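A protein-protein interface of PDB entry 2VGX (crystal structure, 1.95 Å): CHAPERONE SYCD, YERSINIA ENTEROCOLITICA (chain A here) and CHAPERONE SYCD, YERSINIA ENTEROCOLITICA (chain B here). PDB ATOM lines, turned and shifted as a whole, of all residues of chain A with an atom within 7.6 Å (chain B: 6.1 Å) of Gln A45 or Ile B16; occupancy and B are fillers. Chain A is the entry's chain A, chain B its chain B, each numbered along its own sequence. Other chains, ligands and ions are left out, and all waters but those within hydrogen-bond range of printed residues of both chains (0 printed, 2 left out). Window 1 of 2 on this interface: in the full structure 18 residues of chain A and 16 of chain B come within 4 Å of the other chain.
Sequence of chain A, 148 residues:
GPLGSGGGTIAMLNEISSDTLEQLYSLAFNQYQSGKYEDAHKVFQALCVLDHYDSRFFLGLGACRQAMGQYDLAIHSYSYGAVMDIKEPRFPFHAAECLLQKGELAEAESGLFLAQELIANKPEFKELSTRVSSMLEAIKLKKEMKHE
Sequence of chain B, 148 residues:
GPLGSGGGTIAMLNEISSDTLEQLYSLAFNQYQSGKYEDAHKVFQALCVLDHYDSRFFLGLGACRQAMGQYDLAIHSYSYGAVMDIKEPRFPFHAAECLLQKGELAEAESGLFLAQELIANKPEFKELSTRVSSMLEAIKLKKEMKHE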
ATOM      1  N   ALA A  28      25.772 -11.163  -7.214  1.00  0.00           N
ATOM      2  CA  ALA A  28      24.619 -11.530  -6.376  1.00  0.00           C
ATOM      3  C   ALA A  28      23.579 -12.404  -7.127  1.00  0.00           C
ATOM      4  O   ALA A  28      23.022 -13.376  -6.595  1.00  0.00           O
ATOM      5  CB  ALA A  28      23.983 -10.242  -5.786  1.00  0.00           C
ATOM      6  N   GLU A  38      22.054 -17.098   1.156  1.00  0.00           N
ATOM      7  CA  GLU A  38      22.564 -16.269   2.229  1.00  0.00           C
ATOM      8  C   GLU A  38      23.620 -15.333   1.699  1.00  0.00           C
ATOM      9  O   GLU A  38      23.631 -14.143   2.031  1.00  0.00           O
ATOM     10  CB  GLU A  38      23.129 -17.132   3.360  1.00  0.00           C
ATOM     11  CG  GLU A  38      22.132 -18.108   3.995  1.00  0.00           C
ATOM     12  CD  GLU A  38      21.829 -19.373   3.147  1.00  0.00           C
ATOM     13  OE1 GLU A  38      22.508 -19.663   2.120  1.00  0.00           O
ATOM     14  OE2 GLU A  38      20.865 -20.088   3.538  1.00  0.00           O
ATOM     15  N   ASP A  39      24.546 -15.881   0.915  1.00  0.00           N
ATOM     16  CA  ASP A  39      25.628 -15.093   0.381  1.00  0.00           C
ATOM     17  C   ASP A  39      25.091 -14.020  -0.573  1.00  0.00           C
ATOM     18  O   ASP A  39      25.577 -12.903  -0.554  1.00  0.00           O
ATOM     19  CB  ASP A  39      26.624 -15.951  -0.392  1.00  0.00           C
ATOM     20  CG  ASP A  39      27.401 -16.916   0.502  1.00  0.00           C
ATOM     21  OD1 ASP A  39      27.332 -16.819   1.741  1.00  0.00           O
ATOM     22  OD2 ASP A  39      28.075 -17.774  -0.066  1.00  0.00           O
ATOM     23  N   ALA A  40      24.147 -14.386  -1.427  1.00  0.00           N
ATOM     24  CA  ALA A  40      23.511 -13.427  -2.348  1.00  0.00           C
ATOM     25  C   ALA A  40      22.794 -12.330  -1.547  1.00  0.00           C
ATOM     26  O   ALA A  40      22.841 -11.135  -1.885  1.00  0.00           O
ATOM     27  CB  ALA A  40      22.518 -14.141  -3.261  1.00  0.00           C
ATOM     28  N   HIS A  41      22.122 -12.710  -0.472  1.00  0.00           N
ATOM     29  CA  HIS A  41      21.332 -11.717   0.301  1.00  0.00           C
ATOM     30  C   HIS A  41      22.268 -10.600   0.832  1.00  0.00           C
ATOM     31  O   HIS A  41      21.872  -9.447   0.899  1.00  0.00           O
ATOM     32  CB  HIS A  41      20.637 -12.425   1.488  1.00  0.00           C
ATOM     33  CG  HIS A  41      19.783 -11.516   2.337  1.00  0.00           C
ATOM     34  ND1 HIS A  41      20.318 -10.642   3.256  1.00  0.00           N
ATOM     35  CD2 HIS A  41      18.442 -11.359   2.405  1.00  0.00           C
ATOM     36  CE1 HIS A  41      19.344  -9.990   3.864  1.00  0.00           C
ATOM     37  NE2 HIS A  41      18.191 -10.400   3.362  1.00  0.00           N
ATOM     38  N   MLY A  42      23.489 -10.962   1.244  1.00  0.00           N
ATOM     39  CA  MLY A  42      24.438 -10.005   1.813  1.00  0.00           C
ATOM     40  CB  MLY A  42      25.716 -10.684   2.361  1.00  0.00           C
ATOM     41  CG  MLY A  42      25.325 -11.553   3.596  1.00  0.00           C
ATOM     42  CD  MLY A  42      26.396 -12.603   3.946  1.00  0.00           C
ATOM     43  CE  MLY A  42      25.948 -13.136   5.302  1.00  0.00           C
ATOM     44  NZ  MLY A  42      26.327 -14.508   5.607  1.00  0.00           N
ATOM     45  CH1 MLY A  42      26.499 -15.573   4.601  1.00  0.00           C
ATOM     46  CH2 MLY A  42      26.474 -14.809   7.029  1.00  0.00           C
ATOM     47  C   MLY A  42      24.900  -9.026   0.742  1.00  0.00           C
ATOM     48  O   MLY A  42      25.042  -7.864   1.050  1.00  0.00           O
ATOM     49  N   VAL A  43      25.122  -9.482  -0.497  1.00  0.00           N
ATOM     50  CA  VAL A  43      25.468  -8.557  -1.614  1.00  0.00           C
ATOM     51  C   VAL A  43      24.266  -7.669  -1.956  1.00  0.00           C
ATOM     52  O   VAL A  43      24.400  -6.443  -2.199  1.00  0.00           O
ATOM     53  CB  VAL A  43      26.007  -9.324  -2.883  1.00  0.00           C
ATOM     54  CG1 VAL A  43      26.492  -8.329  -3.977  1.00  0.00           C
ATOM     55  CG2 VAL A  43      27.190 -10.156  -2.496  1.00  0.00           C
ATOM     56  N   PHE A  44      23.076  -8.250  -1.953  1.00  0.00           N
ATOM     57  CA  PHE A  44      21.899  -7.421  -2.203  1.00  0.00           C
ATOM     58  C   PHE A  44      21.658  -6.348  -1.106  1.00  0.00           C
ATOM     59  O   PHE A  44      21.252  -5.234  -1.422  1.00  0.00           O
ATOM     60  CB  PHE A  44      20.664  -8.275  -2.390  1.00  0.00           C
ATOM     61  CG  PHE A  44      20.562  -8.912  -3.760  1.00  0.00           C
ATOM     62  CD1 PHE A  44      20.563  -8.137  -4.900  1.00  0.00           C
ATOM     63  CD2 PHE A  44      20.445 -10.285  -3.883  1.00  0.00           C
ATOM     64  CE1 PHE A  44      20.460  -8.735  -6.152  1.00  0.00           C
ATOM     65  CE2 PHE A  44      20.338 -10.895  -5.122  1.00  0.00           C
ATOM     66  CZ  PHE A  44      20.337 -10.108  -6.270  1.00  0.00           C
ATOM     67  N   GLN A  45      21.897  -6.688   0.161  1.00  0.00           N
ATOM     68  CA  GLN A  45      21.895  -5.653   1.246  1.00  0.00           C
ATOM     69  C   GLN A  45      22.814  -4.505   0.918  1.00  0.00           C
ATOM     70  O   GLN A  45      22.431  -3.332   1.049  1.00  0.00           O
ATOM     71  CB  GLN A  45      22.390  -6.244   2.555  1.00  0.00           C
ATOM     72  CG  GLN A  45      21.332  -7.156   3.240  1.00  0.00           C
ATOM     73  CD  GLN A  45      21.874  -7.755   4.536  1.00  0.00           C
ATOM     74  OE1 GLN A  45      22.376  -8.849   4.553  1.00  0.00           O
ATOM     75  NE2 GLN A  45      21.789  -7.002   5.616  1.00  0.00           N
ATOM     76  N   ALA A  46      24.034  -4.837   0.492  1.00  0.00           N
ATOM     77  CA  ALA A  46      24.990  -3.808   0.178  1.00  0.00           C
ATOM     78  C   ALA A  46      24.482  -2.967  -0.987  1.00  0.00           C
ATOM     79  O   ALA A  46      24.590  -1.736  -0.948  1.00  0.00           O
ATOM     80  CB  ALA A  46      26.342  -4.402  -0.157  1.00  0.00           C
ATOM     81  N   LEU A  47      23.967  -3.625  -2.040  1.00  0.00           N
ATOM     82  CA  LEU A  47      23.490  -2.913  -3.255  1.00  0.00           C
ATOM     83  C   LEU A  47      22.315  -1.971  -2.972  1.00  0.00           C
ATOM     84  O   LEU A  47      22.242  -0.863  -3.496  1.00  0.00           O
ATOM     85  CB  LEU A  47      23.055  -3.934  -4.325  1.00  0.00           C
ATOM     86  CG  LEU A  47      24.249  -4.562  -5.049  1.00  0.00           C
ATOM     87  CD1 LEU A  47      23.775  -5.726  -5.968  1.00  0.00           C
ATOM     88  CD2 LEU A  47      24.900  -3.483  -5.880  1.00  0.00           C
ATOM     89  N   CYS A  48      21.384  -2.431  -2.141  1.00  0.00           N
ATOM     90  CA  CYS A  48      20.241  -1.566  -1.667  1.00  0.00           C
ATOM     91  C   CYS A  48      20.657  -0.274  -0.924  1.00  0.00           C
ATOM     92  O   CYS A  48      19.968   0.761  -1.026  1.00  0.00           O
ATOM     93  CB  CYS A  48      19.274  -2.395  -0.792  1.00  0.00           C
ATOM     94  SG  CYS A  48      18.340  -3.673  -1.699  1.00  0.00           S
ATOM     95  N   VAL A  49      21.758  -0.330  -0.173  1.00  0.00           N
ATOM     96  CA  VAL A  49      22.299   0.839   0.511  1.00  0.00           C
ATOM     97  C   VAL A  49      22.970   1.786  -0.520  1.00  0.00           C
ATOM     98  O   VAL A  49      22.819   3.018  -0.452  1.00  0.00           O
ATOM     99  CB  VAL A  49      23.342   0.374   1.611  1.00  0.00           C
ATOM    100  CG1 VAL A  49      24.282   1.522   2.075  1.00  0.00           C
ATOM    101  CG2 VAL A  49      22.589  -0.235   2.776  1.00  0.00           C
ATOM    102  N   LEU A  50      23.674   1.178  -1.479  1.00  0.00           N
ATOM    103  CA  LEU A  50      24.472   1.926  -2.499  1.00  0.00           C
ATOM    104  C   LEU A  50      23.606   2.659  -3.490  1.00  0.00           C
ATOM    105  O   LEU A  50      23.957   3.783  -3.873  1.00  0.00           O
ATOM    106  CB  LEU A  50      25.494   1.026  -3.234  1.00  0.00           C
ATOM    107  CG  LEU A  50      26.655   0.582  -2.295  1.00  0.00           C
ATOM    108  CD1 LEU A  50      27.526  -0.507  -2.924  1.00  0.00           C
ATOM    109  CD2 LEU A  50      27.552   1.726  -1.817  1.00  0.00           C
ATOM    110  N   ASP A  51      22.481   2.045  -3.885  1.00  0.00           N
ATOM    111  CA  ASP A  51      21.533   2.677  -4.803  1.00  0.00           C
ATOM    112  C   ASP A  51      20.135   2.210  -4.432  1.00  0.00           C
ATOM    113  O   ASP A  51      19.711   1.123  -4.848  1.00  0.00           O
ATOM    114  CB  ASP A  51      21.835   2.299  -6.272  1.00  0.00           C
ATOM    115  CG  ASP A  51      21.090   3.217  -7.285  1.00  0.00           C
ATOM    116  OD1 ASP A  51      19.872   3.500  -7.088  1.00  0.00           O
ATOM    117  OD2 ASP A  51      21.733   3.644  -8.291  1.00  0.00           O
ATOM    118  N   PHE A  57      17.440  -4.408  -7.101  1.00  0.00           N
ATOM    119  CA  PHE A  57      18.210  -4.754  -5.858  1.00  0.00           C
ATOM    120  C   PHE A  57      17.219  -5.178  -4.749  1.00  0.00           C
ATOM    121  O   PHE A  57      17.520  -6.045  -3.954  1.00  0.00           O
ATOM    122  CB  PHE A  57      19.150  -3.618  -5.412  1.00  0.00           C
ATOM    123  CG  PHE A  57      20.166  -3.217  -6.473  1.00  0.00           C
ATOM    124  CD1 PHE A  57      20.395  -4.040  -7.578  1.00  0.00           C
ATOM    125  CD2 PHE A  57      20.882  -2.014  -6.361  1.00  0.00           C
ATOM    126  CE1 PHE A  57      21.310  -3.661  -8.580  1.00  0.00           C
ATOM    127  CE2 PHE A  57      21.814  -1.639  -7.344  1.00  0.00           C
ATOM    128  CZ  PHE A  57      22.024  -2.465  -8.440  1.00  0.00           C
ATOM    129  N   PHE A  58      16.035  -4.554  -4.733  1.00  0.00           N
ATOM    130  CA  PHE A  58      14.944  -4.879  -3.809  1.00  0.00           C
ATOM    131  C   PHE A  58      14.171  -6.128  -4.228  1.00  0.00           C
ATOM    132  O   PHE A  58      13.760  -6.904  -3.365  1.00  0.00           O
ATOM    133  CB  PHE A  58      14.046  -3.645  -3.536  1.00  0.00           C
ATOM    134  CG  PHE A  58      14.811  -2.502  -2.926  1.00  0.00           C
ATOM    135  CD1 PHE A  58      14.899  -2.380  -1.536  1.00  0.00           C
ATOM    136  CD2 PHE A  58      15.496  -1.563  -3.734  1.00  0.00           C
ATOM    137  CE1 PHE A  58      15.655  -1.337  -0.935  1.00  0.00           C
ATOM    138  CE2 PHE A  58      16.258  -0.520  -3.142  1.00  0.00           C
ATOM    139  CZ  PHE A  58      16.362  -0.413  -1.763  1.00  0.00           C
ATOM    140  N   GLY A  60      15.820  -8.506  -5.787  1.00  0.00           N
ATOM    141  CA  GLY A  60      16.760  -9.585  -5.414  1.00  0.00           C
ATOM    142  C   GLY A  60      16.794  -9.861  -3.917  1.00  0.00           C
ATOM    143  O   GLY A  60      16.780 -11.022  -3.506  1.00  0.00           O
ATOM    144  N   LEU A  61      16.867  -8.809  -3.100  1.00  0.00           N
ATOM    145  CA  LEU A  61      16.845  -8.975  -1.631  1.00  0.00           C
ATOM    146  C   LEU A  61      15.596  -9.756  -1.236  1.00  0.00           C
ATOM    147  O   LEU A  61      15.649 -10.670  -0.413  1.00  0.00           O
ATOM    148  CB  LEU A  61      16.829  -7.613  -0.904  1.00  0.00           C
ATOM    149  CG  LEU A  61      17.072  -7.637   0.621  1.00  0.00           C
ATOM    150  CD1 LEU A  61      18.578  -7.998   0.896  1.00  0.00           C
ATOM    151  CD2 LEU A  61      16.738  -6.274   1.195  1.00  0.00           C
ATOM    152  N   ARG A  65      15.187 -13.629   0.475  1.00  0.00           N
ATOM    153  CA  ARG A  65      14.400 -13.800   1.700  1.00  0.00           C
ATOM    154  C   ARG A  65      13.286 -14.844   1.514  1.00  0.00           C
ATOM    155  O   ARG A  65      13.059 -15.690   2.375  1.00  0.00           O
ATOM    156  CB  ARG A  65      13.821 -12.463   2.159  1.00  0.00           C
ATOM    157  CG  ARG A  65      14.904 -11.504   2.678  1.00  0.00           C
ATOM    158  CD  ARG A  65      14.445 -10.105   2.887  1.00  0.00           C
ATOM    159  NE  ARG A  65      15.454  -9.319   3.618  1.00  0.00           N
ATOM    160  CZ  ARG A  65      15.247  -8.096   4.103  1.00  0.00           C
ATOM    161  NH1 ARG A  65      14.064  -7.488   3.954  1.00  0.00           N
ATOM    162  NH2 ARG A  65      16.216  -7.485   4.768  1.00  0.00           N
ATOM    163  N   ALA B  11      18.108 -10.163  12.814  1.00  0.00           N
ATOM    164  CA  ALA B  11      18.960  -8.988  12.907  1.00  0.00           C
ATOM    165  C   ALA B  11      20.026  -9.006  11.828  1.00  0.00           C
ATOM    166  O   ALA B  11      20.355  -7.968  11.274  1.00  0.00           O
ATOM    167  CB  ALA B  11      19.609  -8.878  14.285  1.00  0.00           C
ATOM    168  N   MET B  12      20.551 -10.186  11.530  1.00  0.00           N
ATOM    169  CA  MET B  12      21.606 -10.323  10.542  1.00  0.00           C
ATOM    170  C   MET B  12      21.028  -9.971   9.164  1.00  0.00           C
ATOM    171  O   MET B  12      21.721  -9.377   8.354  1.00  0.00           O
ATOM    172  CB  MET B  12      22.199 -11.738  10.587  1.00  0.00           C
ATOM    173  CG  MET B  12      23.187 -12.089   9.495  1.00  0.00           C
ATOM    174  SD  MET B  12      24.816 -11.339   9.703  1.00  0.00           S
ATOM    175  CE  MET B  12      25.405 -11.382   8.022  1.00  0.00           C
ATOM    176  N   LEU B  13      19.763 -10.319   8.913  1.00  0.00           N
ATOM    177  CA  LEU B  13      19.132 -10.021   7.613  1.00  0.00           C
ATOM    178  C   LEU B  13      18.741  -8.561   7.396  1.00  0.00           C
ATOM    179  O   LEU B  13      18.475  -8.143   6.264  1.00  0.00           O
ATOM    180  CB  LEU B  13      17.932 -10.937   7.338  1.00  0.00           C
ATOM    181  CG  LEU B  13      18.222 -12.452   7.306  1.00  0.00           C
ATOM    182  CD1 LEU B  13      16.971 -13.246   6.981  1.00  0.00           C
ATOM    183  CD2 LEU B  13      19.337 -12.807   6.313  1.00  0.00           C
ATOM    184  N   ASN B  14      18.694  -7.800   8.478  1.00  0.00           N
ATOM    185  CA  ASN B  14      18.259  -6.398   8.447  1.00  0.00           C
ATOM    186  C   ASN B  14      19.361  -5.356   8.589  1.00  0.00           C
ATOM    187  O   ASN B  14      19.107  -4.169   8.420  1.00  0.00           O
ATOM    188  CB  ASN B  14      17.242  -6.175   9.565  1.00  0.00           C
ATOM    189  CG  ASN B  14      15.844  -6.505   9.130  1.00  0.00           C
ATOM    190  OD1 ASN B  14      15.368  -5.992   8.117  1.00  0.00           O
ATOM    191  ND2 ASN B  14      15.178  -7.366   9.881  1.00  0.00           N
ATOM    192  N   GLU B  15      20.570  -5.792   8.904  1.00  0.00           N
ATOM    193  CA  GLU B  15      21.663  -4.877   9.191  1.00  0.00           C
ATOM    194  C   GLU B  15      22.884  -5.275   8.441  1.00  0.00           C
ATOM    195  O   GLU B  15      23.119  -6.455   8.258  1.00  0.00           O
ATOM    196  CB  GLU B  15      22.048  -4.932  10.685  1.00  0.00           C
ATOM    197  CG  GLU B  15      20.923  -4.647  11.615  1.00  0.00           C
ATOM    198  CD  GLU B  15      21.366  -4.423  13.050  1.00  0.00           C
ATOM    199  OE1 GLU B  15      22.456  -4.907  13.456  1.00  0.00           O
ATOM    200  OE2 GLU B  15      20.597  -3.743  13.770  1.00  0.00           O
ATOM    201  N   ILE B  16      23.664  -4.277   8.021  1.00  0.00           N
ATOM    202  CA  ILE B  16      25.001  -4.484   7.491  1.00  0.00           C
ATOM    203  C   ILE B  16      25.973  -4.547   8.684  1.00  0.00           C
ATOM    204  O   ILE B  16      26.057  -3.587   9.442  1.00  0.00           O
ATOM    205  CB  ILE B  16      25.408  -3.289   6.619  1.00  0.00           C
ATOM    206  CG1 ILE B  16      24.333  -2.954   5.558  1.00  0.00           C
ATOM    207  CG2 ILE B  16      26.828  -3.475   6.045  1.00  0.00           C
ATOM    208  CD1 ILE B  16      24.206  -3.933   4.514  1.00  0.00           C
ATOM    209  N   SER B  17      26.682  -5.665   8.846  1.00  0.00           N
ATOM    210  CA  SER B  17      27.738  -5.819   9.837  1.00  0.00           C
ATOM    211  C   SER B  17      28.998  -6.220   9.092  1.00  0.00           C
ATOM    212  O   SER B  17      28.948  -6.468   7.881  1.00  0.00           O
ATOM    213  CB  SER B  17      27.346  -6.930  10.830  1.00  0.00           C
ATOM    214  OG  SER B  17      27.237  -8.179  10.163  1.00  0.00           O
ATOM    215  N   SER B  18      30.130  -6.319   9.790  1.00  0.00           N
ATOM    216  CA  SER B  18      31.343  -6.840   9.147  1.00  0.00           C
ATOM    217  C   SER B  18      31.101  -8.230   8.542  1.00  0.00           C
ATOM    218  O   SER B  18      31.639  -8.552   7.485  1.00  0.00           O
ATOM    219  CB  SER B  18      32.506  -6.892  10.148  1.00  0.00           C
ATOM    220  OG  SER B  18      32.837  -5.565  10.532  1.00  0.00           O
ATOM    221  N   THR B  20      28.375  -9.314   7.068  1.00  0.00           N
ATOM    222  CA  THR B  20      27.743  -9.081   5.776  1.00  0.00           C
ATOM    223  C   THR B  20      28.798  -8.891   4.678  1.00  0.00           C
ATOM    224  O   THR B  20      28.567  -9.285   3.529  1.00  0.00           O
ATOM    225  CB  THR B  20      26.858  -7.803   5.802  1.00  0.00           C
ATOM    226  OG1 THR B  20      26.041  -7.782   6.997  1.00  0.00           O
ATOM    227  CG2 THR B  20      25.997  -7.682   4.532  1.00  0.00           C
ATOM    228  N   LEU B  21      29.950  -8.303   5.035  1.00  0.00           N
ATOM    229  CA  LEU B  21      30.933  -7.835   4.034  1.00  0.00           C
ATOM    230  C   LEU B  21      32.122  -8.796   3.842  1.00  0.00           C
ATOM    231  O   LEU B  21      32.961  -8.597   2.948  1.00  0.00           O
ATOM    232  CB  LEU B  21      31.434  -6.412   4.413  1.00  0.00           C
ATOM    233  CG  LEU B  21      30.338  -5.353   4.666  1.00  0.00           C
ATOM    234  CD1 LEU B  21      30.975  -4.067   5.137  1.00  0.00           C
ATOM    235  CD2 LEU B  21      29.471  -5.090   3.410  1.00  0.00           C
ATOM    236  N   LEU B  50      30.695   1.214   2.419  1.00  0.00           N
ATOM    237  CA  LEU B  50      29.810   0.435   3.287  1.00  0.00           C
ATOM    238  C   LEU B  50      30.246   0.434   4.737  1.00  0.00           C
ATOM    239  O   LEU B  50      29.394   0.441   5.624  1.00  0.00           O
ATOM    240  CB  LEU B  50      29.609  -0.987   2.742  1.00  0.00           C
ATOM    241  CG  LEU B  50      28.844  -1.095   1.405  1.00  0.00           C
ATOM    242  CD1 LEU B  50      29.249  -2.358   0.570  1.00  0.00           C
ATOM    243  CD2 LEU B  50      27.316  -0.990   1.604  1.00  0.00           C
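Printed residues of chain B within 4 Å of His A41: Leu B13 (3.2 Å). Of the printed residues of chain B, MLY A42 touches Met B12 and Thr B20. Of chain B, only Met B12 (3.6 Å), Leu B13 (3.6 Å), Glu B15 (3.0 Å), Ile B16 (3.5 Å) and Thr B20 (3.8 Å) come within 4 Å of Gln A45. Printed residues of chain B within 4 Å of Val A49: Leu B50 (3.97 Å). Phe A57 touches none of the printed residues of chain B. Printed residues of chain A within 4 Å of Leu B13: His A41 (3.2 Å), Gln A45 (3.6 Å) and Arg A65 (2.8 Å). Printed residues of chain A within 4 Å of Glu B15: Gln A45 (3.0 Å). Of chain A, only Gln A45 comes within 4 Å of Ile B16. Ser B18 touches none of the printed residues of chain A. The nearest residue of chain B that does not touch Gln A45 is Asn B14 (4.2 Å). The nearest residue of chain A that does not touch Ile B16 is Ala A46 (4.1 Å). The nearest printed residue of chain A that does not touch Thr B20 is Val A43 (5.3 Å).
Of the 20 printed residues of chain A, 6 touch a printed residue of chain B. Hydrophobic or aromatic side chains of chain A within 4 Å of the printed part of chain B: His A41, Ala A46 and Val A49. Among the printed residues, 12 pairs touch across the chains. Among the printed residues, no Asp or Glu carboxylate lies within 4 Å of a Lys or Arg side-chain nitrogen of the other chain.
A ring nitrogen (ND1) of His A41 is in hydrogen-bond range of the side-chain amide oxygen (OE1) of Gln A45, 3.0 Å away. O of Glu B15 sits at hydrogen-bond distance from OG1 of Thr B20, at 3.4 Å. NE2 of His A41 sits at hydrogen-bond distance from NE of Arg A65 (3.0 Å). N of Ser B17 sits at hydrogen-bond distance from OG1 of Thr B20 (2.9 Å).
Among the printed residues, pairs that only touch across the chains: His A41 with Leu B13, MLY A42 with Met B12, MLY A42 with Thr B20, Gln A45 with Ile B16, Gln A45 with Leu B13, Gln A45 with Met B12, Ala A46 with Leu B50, Arg A65 with Asn B14, Gln A45 with Thr B20 and Val A49 with Leu B50.
The guanidinium group (NH2) of Arg A65 sits at hydrogen-bond distance from the backbone carbonyl oxygen (O) of Leu B13 (2.8 Å). The backbone carbonyl oxygen (O) of Glu B15 sits at hydrogen-bond distance from the side-chain amide nitrogen (NE2) of Gln A45 (3.0 Å).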
